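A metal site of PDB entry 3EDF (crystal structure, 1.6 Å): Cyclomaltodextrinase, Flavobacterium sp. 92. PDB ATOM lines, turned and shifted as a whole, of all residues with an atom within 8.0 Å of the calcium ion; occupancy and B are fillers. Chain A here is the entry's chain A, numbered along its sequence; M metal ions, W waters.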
ATOM      1  N   PRO A 114      15.659  -0.258  -8.445  1.00  0.00           N
ATOM      2  CA  PRO A 114      14.882  -0.657  -9.644  1.00  0.00           C
ATOM      3  C   PRO A 114      13.359  -0.705  -9.366  1.00  0.00           C
ATOM      4  O   PRO A 114      12.583  -0.283 -10.217  1.00  0.00           O
ATOM      5  CB  PRO A 114      15.445  -2.035 -10.013  1.00  0.00           C
ATOM      6  CG  PRO A 114      16.273  -2.478  -8.826  1.00  0.00           C
ATOM      7  CD  PRO A 114      16.751  -1.212  -8.163  1.00  0.00           C
ATOM      8  N   ASP A 115      12.947  -1.157  -8.200  1.00  0.00           N
ATOM      9  CA  ASP A 115      11.471  -1.171  -7.911  1.00  0.00           C
ATOM     10  C   ASP A 115      10.859   0.236  -7.807  1.00  0.00           C
ATOM     11  O   ASP A 115       9.619   0.382  -7.920  1.00  0.00           O
ATOM     12  CB  ASP A 115      11.207  -1.903  -6.591  1.00  0.00           C
ATOM     13  CG  ASP A 115       9.704  -2.023  -6.288  1.00  0.00           C
ATOM     14  OD1 ASP A 115       9.288  -1.471  -5.230  1.00  0.00           O
ATOM     15  OD2 ASP A 115       9.005  -2.594  -7.130  1.00  0.00           O
ATOM     16  N   ALA A 118      11.186   3.290 -12.326  1.00  0.00           N
ATOM     17  CA  ALA A 118      10.206   3.405 -13.423  1.00  0.00           C
ATOM     18  C   ALA A 118       9.540   2.070 -13.715  1.00  0.00           C
ATOM     19  O   ALA A 118      10.204   1.079 -13.908  1.00  0.00           O
ATOM     20  CB  ALA A 118      10.877   4.002 -14.688  1.00  0.00           C
ATOM     21  N   ASN A 119       8.214   2.081 -13.725  1.00  0.00           N
ATOM     22  CA  ASN A 119       7.409   0.894 -13.980  1.00  0.00           C
ATOM     23  C   ASN A 119       7.053   0.850 -15.465  1.00  0.00           C
ATOM     24  O   ASN A 119       6.038   1.378 -15.908  1.00  0.00           O
ATOM     25  CB  ASN A 119       6.168   0.875 -13.076  1.00  0.00           C
ATOM     26  CG  ASN A 119       5.365  -0.413 -13.200  1.00  0.00           C
ATOM     27  OD1 ASN A 119       5.672  -1.258 -14.042  1.00  0.00           O
ATOM     28  ND2 ASN A 119       4.309  -0.571 -12.360  1.00  0.00           N
ATOM     29  N   GLY A 120       7.952   0.267 -16.262  1.00  0.00           N
ATOM     30  CA  GLY A 120       7.770   0.206 -17.700  1.00  0.00           C
ATOM     31  C   GLY A 120       6.776  -0.853 -18.151  1.00  0.00           C
ATOM     32  O   GLY A 120       6.299  -0.815 -19.308  1.00  0.00           O
ATOM     33  N   ASP A 121       6.491  -1.800 -17.258  1.00  0.00           N
ATOM     34  CA  ASP A 121       5.584  -2.897 -17.592  1.00  0.00           C
ATOM     35  C   ASP A 121       4.781  -3.246 -16.348  1.00  0.00           C
ATOM     36  O   ASP A 121       5.261  -3.975 -15.495  1.00  0.00           O
ATOM     37  CB  ASP A 121       6.400  -4.101 -18.038  1.00  0.00           C
ATOM     38  CG  ASP A 121       5.525  -5.259 -18.494  1.00  0.00           C
ATOM     39  OD1 ASP A 121       4.277  -5.179 -18.376  1.00  0.00           O
ATOM     40  OD2 ASP A 121       6.113  -6.229 -18.988  1.00  0.00           O
ATOM     41  N   PRO A 122       3.574  -2.667 -16.200  1.00  0.00           N
ATOM     42  CA  PRO A 122       2.786  -3.019 -15.013  1.00  0.00           C
ATOM     43  C   PRO A 122       2.413  -4.500 -14.930  1.00  0.00           C
ATOM     44  O   PRO A 122       2.072  -4.967 -13.849  1.00  0.00           O
ATOM     45  CB  PRO A 122       1.523  -2.146 -15.166  1.00  0.00           C
ATOM     46  CG  PRO A 122       1.984  -1.006 -16.017  1.00  0.00           C
ATOM     47  CD  PRO A 122       2.915  -1.629 -17.005  1.00  0.00           C
ATOM     48  N   SER A 123       2.522  -5.214 -16.026  1.00  0.00           N
ATOM     49  CA  SER A 123       2.098  -6.622 -16.058  1.00  0.00           C
ATOM     50  C   SER A 123       3.044  -7.558 -15.297  1.00  0.00           C
ATOM     51  O   SER A 123       2.660  -8.690 -14.994  1.00  0.00           O
ATOM     52  CB  SER A 123       1.886  -7.143 -17.476  1.00  0.00           C
ATOM     53  OG  SER A 123       3.097  -7.507 -18.101  1.00  0.00           O
ATOM     54  N   ASN A 124       4.272  -7.120 -15.024  1.00  0.00           N
ATOM     55  CA  ASN A 124       5.161  -7.968 -14.214  1.00  0.00           C
ATOM     56  C   ASN A 124       5.216  -7.542 -12.757  1.00  0.00           C
ATOM     57  O   ASN A 124       6.045  -8.064 -11.988  1.00  0.00           O
ATOM     58  CB  ASN A 124       6.573  -8.063 -14.810  1.00  0.00           C
ATOM     59  CG  ASN A 124       7.267  -6.714 -14.890  1.00  0.00           C
ATOM     60  OD1 ASN A 124       6.919  -5.779 -14.188  1.00  0.00           O
ATOM     61  ND2 ASN A 124       8.254  -6.627 -15.800  1.00  0.00           N
ATOM     62  N   ASP A 125       4.340  -6.607 -12.365  1.00  0.00           N
ATOM     63  CA  ASP A 125       4.325  -6.115 -10.986  1.00  0.00           C
ATOM     64  C   ASP A 125       4.142  -7.281 -10.014  1.00  0.00           C
ATOM     65  O   ASP A 125       4.733  -7.317  -8.929  1.00  0.00           O
ATOM     66  CB  ASP A 125       3.231  -5.060 -10.775  1.00  0.00           C
ATOM     67  CG  ASP A 125       3.534  -3.758 -11.478  1.00  0.00           C
ATOM     68  OD1 ASP A 125       4.567  -3.688 -12.213  1.00  0.00           O
ATOM     69  OD2 ASP A 125       2.751  -2.789 -11.318  1.00  0.00           O
ATOM     70  N   ASN A 126       3.280  -8.207 -10.441  1.00  0.00           N
ATOM     71  CA  ASN A 126       3.104  -9.511  -9.815  1.00  0.00           C
ATOM     72  C   ASN A 126       3.463 -10.603 -10.801  1.00  0.00           C
ATOM     73  O   ASN A 126       3.204 -10.472 -12.005  1.00  0.00           O
ATOM     74  CB  ASN A 126       1.644  -9.701  -9.363  1.00  0.00           C
ATOM     75  CG  ASN A 126       1.236  -8.687  -8.341  1.00  0.00           C
ATOM     76  OD1 ASN A 126       1.938  -8.480  -7.360  1.00  0.00           O
ATOM     77  ND2 ASN A 126       0.095  -8.040  -8.552  1.00  0.00           N
ATOM     78  N   ALA A 134       2.288  -6.886  -5.181  1.00  0.00           N
ATOM     79  CA  ALA A 134       2.661  -5.466  -5.236  1.00  0.00           C
ATOM     80  C   ALA A 134       1.683  -4.598  -4.459  1.00  0.00           C
ATOM     81  O   ALA A 134       0.472  -4.900  -4.369  1.00  0.00           O
ATOM     82  CB  ALA A 134       2.759  -4.969  -6.676  1.00  0.00           C
ATOM     83  N   ARG A 142       6.306  -3.758  -2.728  1.00  0.00           N
ATOM     84  CA  ARG A 142       6.752  -3.639  -4.129  1.00  0.00           C
ATOM     85  C   ARG A 142       5.876  -2.620  -4.881  1.00  0.00           C
ATOM     86  O   ARG A 142       4.643  -2.720  -4.896  1.00  0.00           O
ATOM     87  CB  ARG A 142       6.743  -4.980  -4.877  1.00  0.00           C
ATOM     88  CG  ARG A 142       7.640  -6.013  -4.287  1.00  0.00           C
ATOM     89  CD  ARG A 142       7.757  -7.182  -5.238  1.00  0.00           C
ATOM     90  NE  ARG A 142       8.566  -6.819  -6.405  1.00  0.00           N
ATOM     91  CZ  ARG A 142       9.887  -6.949  -6.448  1.00  0.00           C
ATOM     92  NH1 ARG A 142      10.548  -6.582  -7.554  1.00  0.00           N
ATOM     93  NH2 ARG A 142      10.534  -7.464  -5.404  1.00  0.00           N
ATOM     94  N   HIS A 143       6.513  -1.645  -5.522  1.00  0.00           N
ATOM     95  CA  HIS A 143       5.772  -0.627  -6.278  1.00  0.00           C
ATOM     96  C   HIS A 143       5.658  -0.898  -7.781  1.00  0.00           C
ATOM     97  O   HIS A 143       4.781  -0.354  -8.471  1.00  0.00           O
ATOM     98  CB  HIS A 143       6.369   0.752  -5.994  1.00  0.00           C
ATOM     99  CG  HIS A 143       6.223   1.163  -4.564  1.00  0.00           C
ATOM    100  ND1 HIS A 143       6.572   2.415  -4.111  1.00  0.00           N
ATOM    101  CD2 HIS A 143       5.764   0.485  -3.489  1.00  0.00           C
ATOM    102  CE1 HIS A 143       6.356   2.483  -2.813  1.00  0.00           C
ATOM    103  NE2 HIS A 143       5.867   1.325  -2.404  1.00  0.00           N
ATOM    104  N   GLY A 144       6.562  -1.741  -8.286  1.00  0.00           N
ATOM    105  CA  GLY A 144       6.479  -2.251  -9.654  1.00  0.00           C
ATOM    106  C   GLY A 144       7.540  -1.746 -10.621  1.00  0.00           C
ATOM    107  O   GLY A 144       7.427  -1.958 -11.833  1.00  0.00           O
ATOM    108  N   GLY A 145       8.571  -1.058 -10.114  1.00  0.00           N
ATOM    109  CA  GLY A 145       9.626  -0.571 -11.027  1.00  0.00           C
ATOM    110  C   GLY A 145      10.303  -1.796 -11.669  1.00  0.00           C
ATOM    111  O   GLY A 145      10.407  -2.842 -11.064  1.00  0.00           O
ATOM    112  N   ASP A 146      10.812  -1.648 -12.890  1.00  0.00           N
ATOM    113  CA  ASP A 146      11.403  -2.794 -13.563  1.00  0.00           C
ATOM    114  C   ASP A 146      12.487  -2.403 -14.561  1.00  0.00           C
ATOM    115  O   ASP A 146      12.780  -1.199 -14.756  1.00  0.00           O
ATOM    116  CB  ASP A 146      10.286  -3.603 -14.253  1.00  0.00           C
ATOM    117  CG  ASP A 146       9.372  -2.700 -15.084  1.00  0.00           C
ATOM    118  OD1 ASP A 146       8.112  -2.880 -15.047  1.00  0.00           O
ATOM    119  OD2 ASP A 146       9.908  -1.785 -15.748  1.00  0.00           O
ATOM    120  N   ILE A 147      13.082  -3.420 -15.190  1.00  0.00           N
ATOM    121  CA  ILE A 147      14.168  -3.180 -16.184  1.00  0.00           C
ATOM    122  C   ILE A 147      13.637  -2.382 -17.405  1.00  0.00           C
ATOM    123  O   ILE A 147      14.321  -1.468 -17.876  1.00  0.00           O
ATOM    124  CB  ILE A 147      14.842  -4.489 -16.625  1.00  0.00           C
ATOM    125  CG1 ILE A 147      15.672  -5.065 -15.466  1.00  0.00           C
ATOM    126  CG2 ILE A 147      15.670  -4.261 -17.927  1.00  0.00           C
ATOM    127  CD1 ILE A 147      16.108  -6.521 -15.646  1.00  0.00           C
ATOM    128  N   ARG A 148      12.447  -2.724 -17.900  1.00  0.00           N
ATOM    129  CA  ARG A 148      11.846  -1.969 -18.994  1.00  0.00           C
ATOM    130  C   ARG A 148      11.801  -0.464 -18.708  1.00  0.00           C
ATOM    131  O   ARG A 148      12.222   0.361 -19.549  1.00  0.00           O
ATOM    132  CB  ARG A 148      10.455  -2.514 -19.343  1.00  0.00           C
ATOM    133  CG  ARG A 148       9.844  -1.775 -20.557  1.00  0.00           C
ATOM    134  CD  ARG A 148       8.635  -2.556 -21.094  1.00  0.00           C
ATOM    135  NE  ARG A 148       7.918  -1.826 -22.140  1.00  0.00           N
ATOM    136  CZ  ARG A 148       6.764  -2.212 -22.666  1.00  0.00           C
ATOM    137  NH1 ARG A 148       6.176  -1.472 -23.610  1.00  0.00           N
ATOM    138  NH2 ARG A 148       6.177  -3.338 -22.265  1.00  0.00           N
ATOM    139  N   GLY A 149      11.333  -0.100 -17.503  1.00  0.00           N
ATOM    140  CA  GLY A 149      11.226   1.309 -17.106  1.00  0.00           C
ATOM    141  C   GLY A 149      12.601   1.979 -17.047  1.00  0.00           C
ATOM    142  O   GLY A 149      12.766   3.125 -17.457  1.00  0.00           O
ATOM    143  N   PRO A 193      11.851 -12.114 -11.445  1.00  0.00           N
ATOM    144  CA  PRO A 193      10.988 -11.970 -12.626  1.00  0.00           C
ATOM    145  C   PRO A 193      10.110 -10.719 -12.631  1.00  0.00           C
ATOM    146  O   PRO A 193       9.588 -10.300 -13.687  1.00  0.00           O
ATOM    147  CB  PRO A 193      10.072 -13.226 -12.569  1.00  0.00           C
ATOM    148  CG  PRO A 193      10.649 -14.140 -11.602  1.00  0.00           C
ATOM    149  CD  PRO A 193      11.696 -13.425 -10.765  1.00  0.00           C
ATOM    150  N   ARG A 194       9.966 -10.104 -11.471  1.00  0.00           N
ATOM    151  CA  ARG A 194       9.205  -8.877 -11.411  1.00  0.00           C
ATOM    152  C   ARG A 194       9.977  -7.736 -12.063  1.00  0.00           C
ATOM    153  O   ARG A 194       9.385  -6.745 -12.439  1.00  0.00           O
ATOM    154  CB  ARG A 194       8.756  -8.599  -9.989  1.00  0.00           C
ATOM    155  CG  ARG A 194       7.701  -9.668  -9.615  1.00  0.00           C
ATOM    156  CD  ARG A 194       7.473  -9.723  -8.167  1.00  0.00           C
ATOM    157  NE  ARG A 194       8.666 -10.140  -7.394  1.00  0.00           N
ATOM    158  CZ  ARG A 194       8.593 -10.540  -6.133  1.00  0.00           C
ATOM    159  NH1 ARG A 194       7.398 -10.545  -5.520  1.00  0.00           N
ATOM    160  NH2 ARG A 194       9.692 -10.902  -5.488  1.00  0.00           N
ATOM    161  N   TYR A 195      11.299  -7.891 -12.196  1.00  0.00           N
ATOM    162  CA  TYR A 195      12.110  -6.858 -12.864  1.00  0.00           C
ATOM    163  C   TYR A 195      12.232  -7.196 -14.349  1.00  0.00           C
ATOM    164  O   TYR A 195      12.356  -6.295 -15.172  1.00  0.00           O
ATOM    165  CB  TYR A 195      13.514  -6.755 -12.241  1.00  0.00           C
ATOM    166  CG  TYR A 195      13.484  -6.210 -10.825  1.00  0.00           C
ATOM    167  CD1 TYR A 195      12.785  -5.049 -10.520  1.00  0.00           C
ATOM    168  CD2 TYR A 195      14.152  -6.877  -9.790  1.00  0.00           C
ATOM    169  CE1 TYR A 195      12.737  -4.544  -9.227  1.00  0.00           C
ATOM    170  CE2 TYR A 195      14.127  -6.383  -8.470  1.00  0.00           C
ATOM    171  CZ  TYR A 195      13.422  -5.201  -8.214  1.00  0.00           C
ATOM    172  OH  TYR A 195      13.352  -4.697  -6.951  1.00  0.00           O
ATOM    173  N   GLY A 196      12.260  -8.493 -14.639  1.00  0.00           N
ATOM    174  CA  GLY A 196      12.372  -9.007 -16.020  1.00  0.00           C
ATOM    175  C   GLY A 196      13.216 -10.267 -16.030  1.00  0.00           C
ATOM    176  O   GLY A 196      13.339 -10.949 -15.019  1.00  0.00           O
ATOM    177  N   TRP A 477       5.666   6.212 -13.171  1.00  0.00           N
ATOM    178  CA  TRP A 477       4.419   5.448 -13.198  1.00  0.00           C
ATOM    179  C   TRP A 477       3.402   6.177 -14.049  1.00  0.00           C
ATOM    180  O   TRP A 477       3.253   7.392 -13.939  1.00  0.00           O
ATOM    181  CB  TRP A 477       3.832   5.253 -11.791  1.00  0.00           C
ATOM    182  CG  TRP A 477       4.408   4.084 -11.065  1.00  0.00           C
ATOM    183  CD1 TRP A 477       3.790   2.890 -10.796  1.00  0.00           C
ATOM    184  CD2 TRP A 477       5.739   3.983 -10.518  1.00  0.00           C
ATOM    185  NE1 TRP A 477       4.656   2.051 -10.120  1.00  0.00           N
ATOM    186  CE2 TRP A 477       5.861   2.690  -9.952  1.00  0.00           C
ATOM    187  CE3 TRP A 477       6.846   4.861 -10.469  1.00  0.00           C
ATOM    188  CZ2 TRP A 477       7.042   2.255  -9.343  1.00  0.00           C
ATOM    189  CZ3 TRP A 477       8.042   4.409  -9.869  1.00  0.00           C
ATOM    190  CH2 TRP A 477       8.117   3.115  -9.299  1.00  0.00           C
HETATM  191 CA    CA M   1       6.506  -3.533 -13.456  1.00  0.00          CA
HETATM  192  O   HOH W   1       7.710  -4.858 -11.601  1.00  0.00           O
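OD1 of Asn 124 sits close to O of Arg 194.
The side-chain carboxylate of Asp 146 lies within hydrogen-bond range of the backbone NH of Gly 120, 2.9 Å away.
The side-chain carboxylate (OD2) of Asp 146 sits close to the backbone NH (N) of Arg 148 (3.5 Å).
The side-chain carboxylate (OD1) of Asp 121 is in hydrogen-bond range of the side-chain hydroxyl (OG) of Ser 123 (2.6 Å).
The side-chain carboxylate (OD2) of Asp 146 sits at hydrogen-bond distance from the backbone NH (N) of Gly 149, 2.8 Å away.
O of Ala 118 is in hydrogen-bond range of N of Asp 146, 3.0 Å away.
The backbone carbonyl oxygen (O) of Pro 114 sits at hydrogen-bond distance from the backbone NH (N) of Asp 146, at 3.5 Å.
The backbone NH of Gly 144 lies within hydrogen-bond range of the side-chain carboxylate of Asp 115.
Water W1 bridges O of Arg 194 and O of Gly 145.
OD1 of Asp 125 binds the calcium ion, at 2.3 Å.
The calcium ion is bound by the side-chain carboxylate (OD1) of Asp 146 (2.4 Å).
The calcium ion is bound by OD1 of Asn 124, at 2.4 Å.
O of Asp 121 is bound to the calcium ion.
The calcium ion is bound by O of Gly 144, 2.4 Å away.
OD1 of Asn 119 binds the calcium ion.
Water W1 binds the calcium ion, at 2.6 Å.
The calcium ion has seven donor atoms within binding distance.
Six residues have an atom within 4 Å of the calcium ion: Asn 119, Asp 121, Asn 124, Asp 125, Gly 144 and Asp 146.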
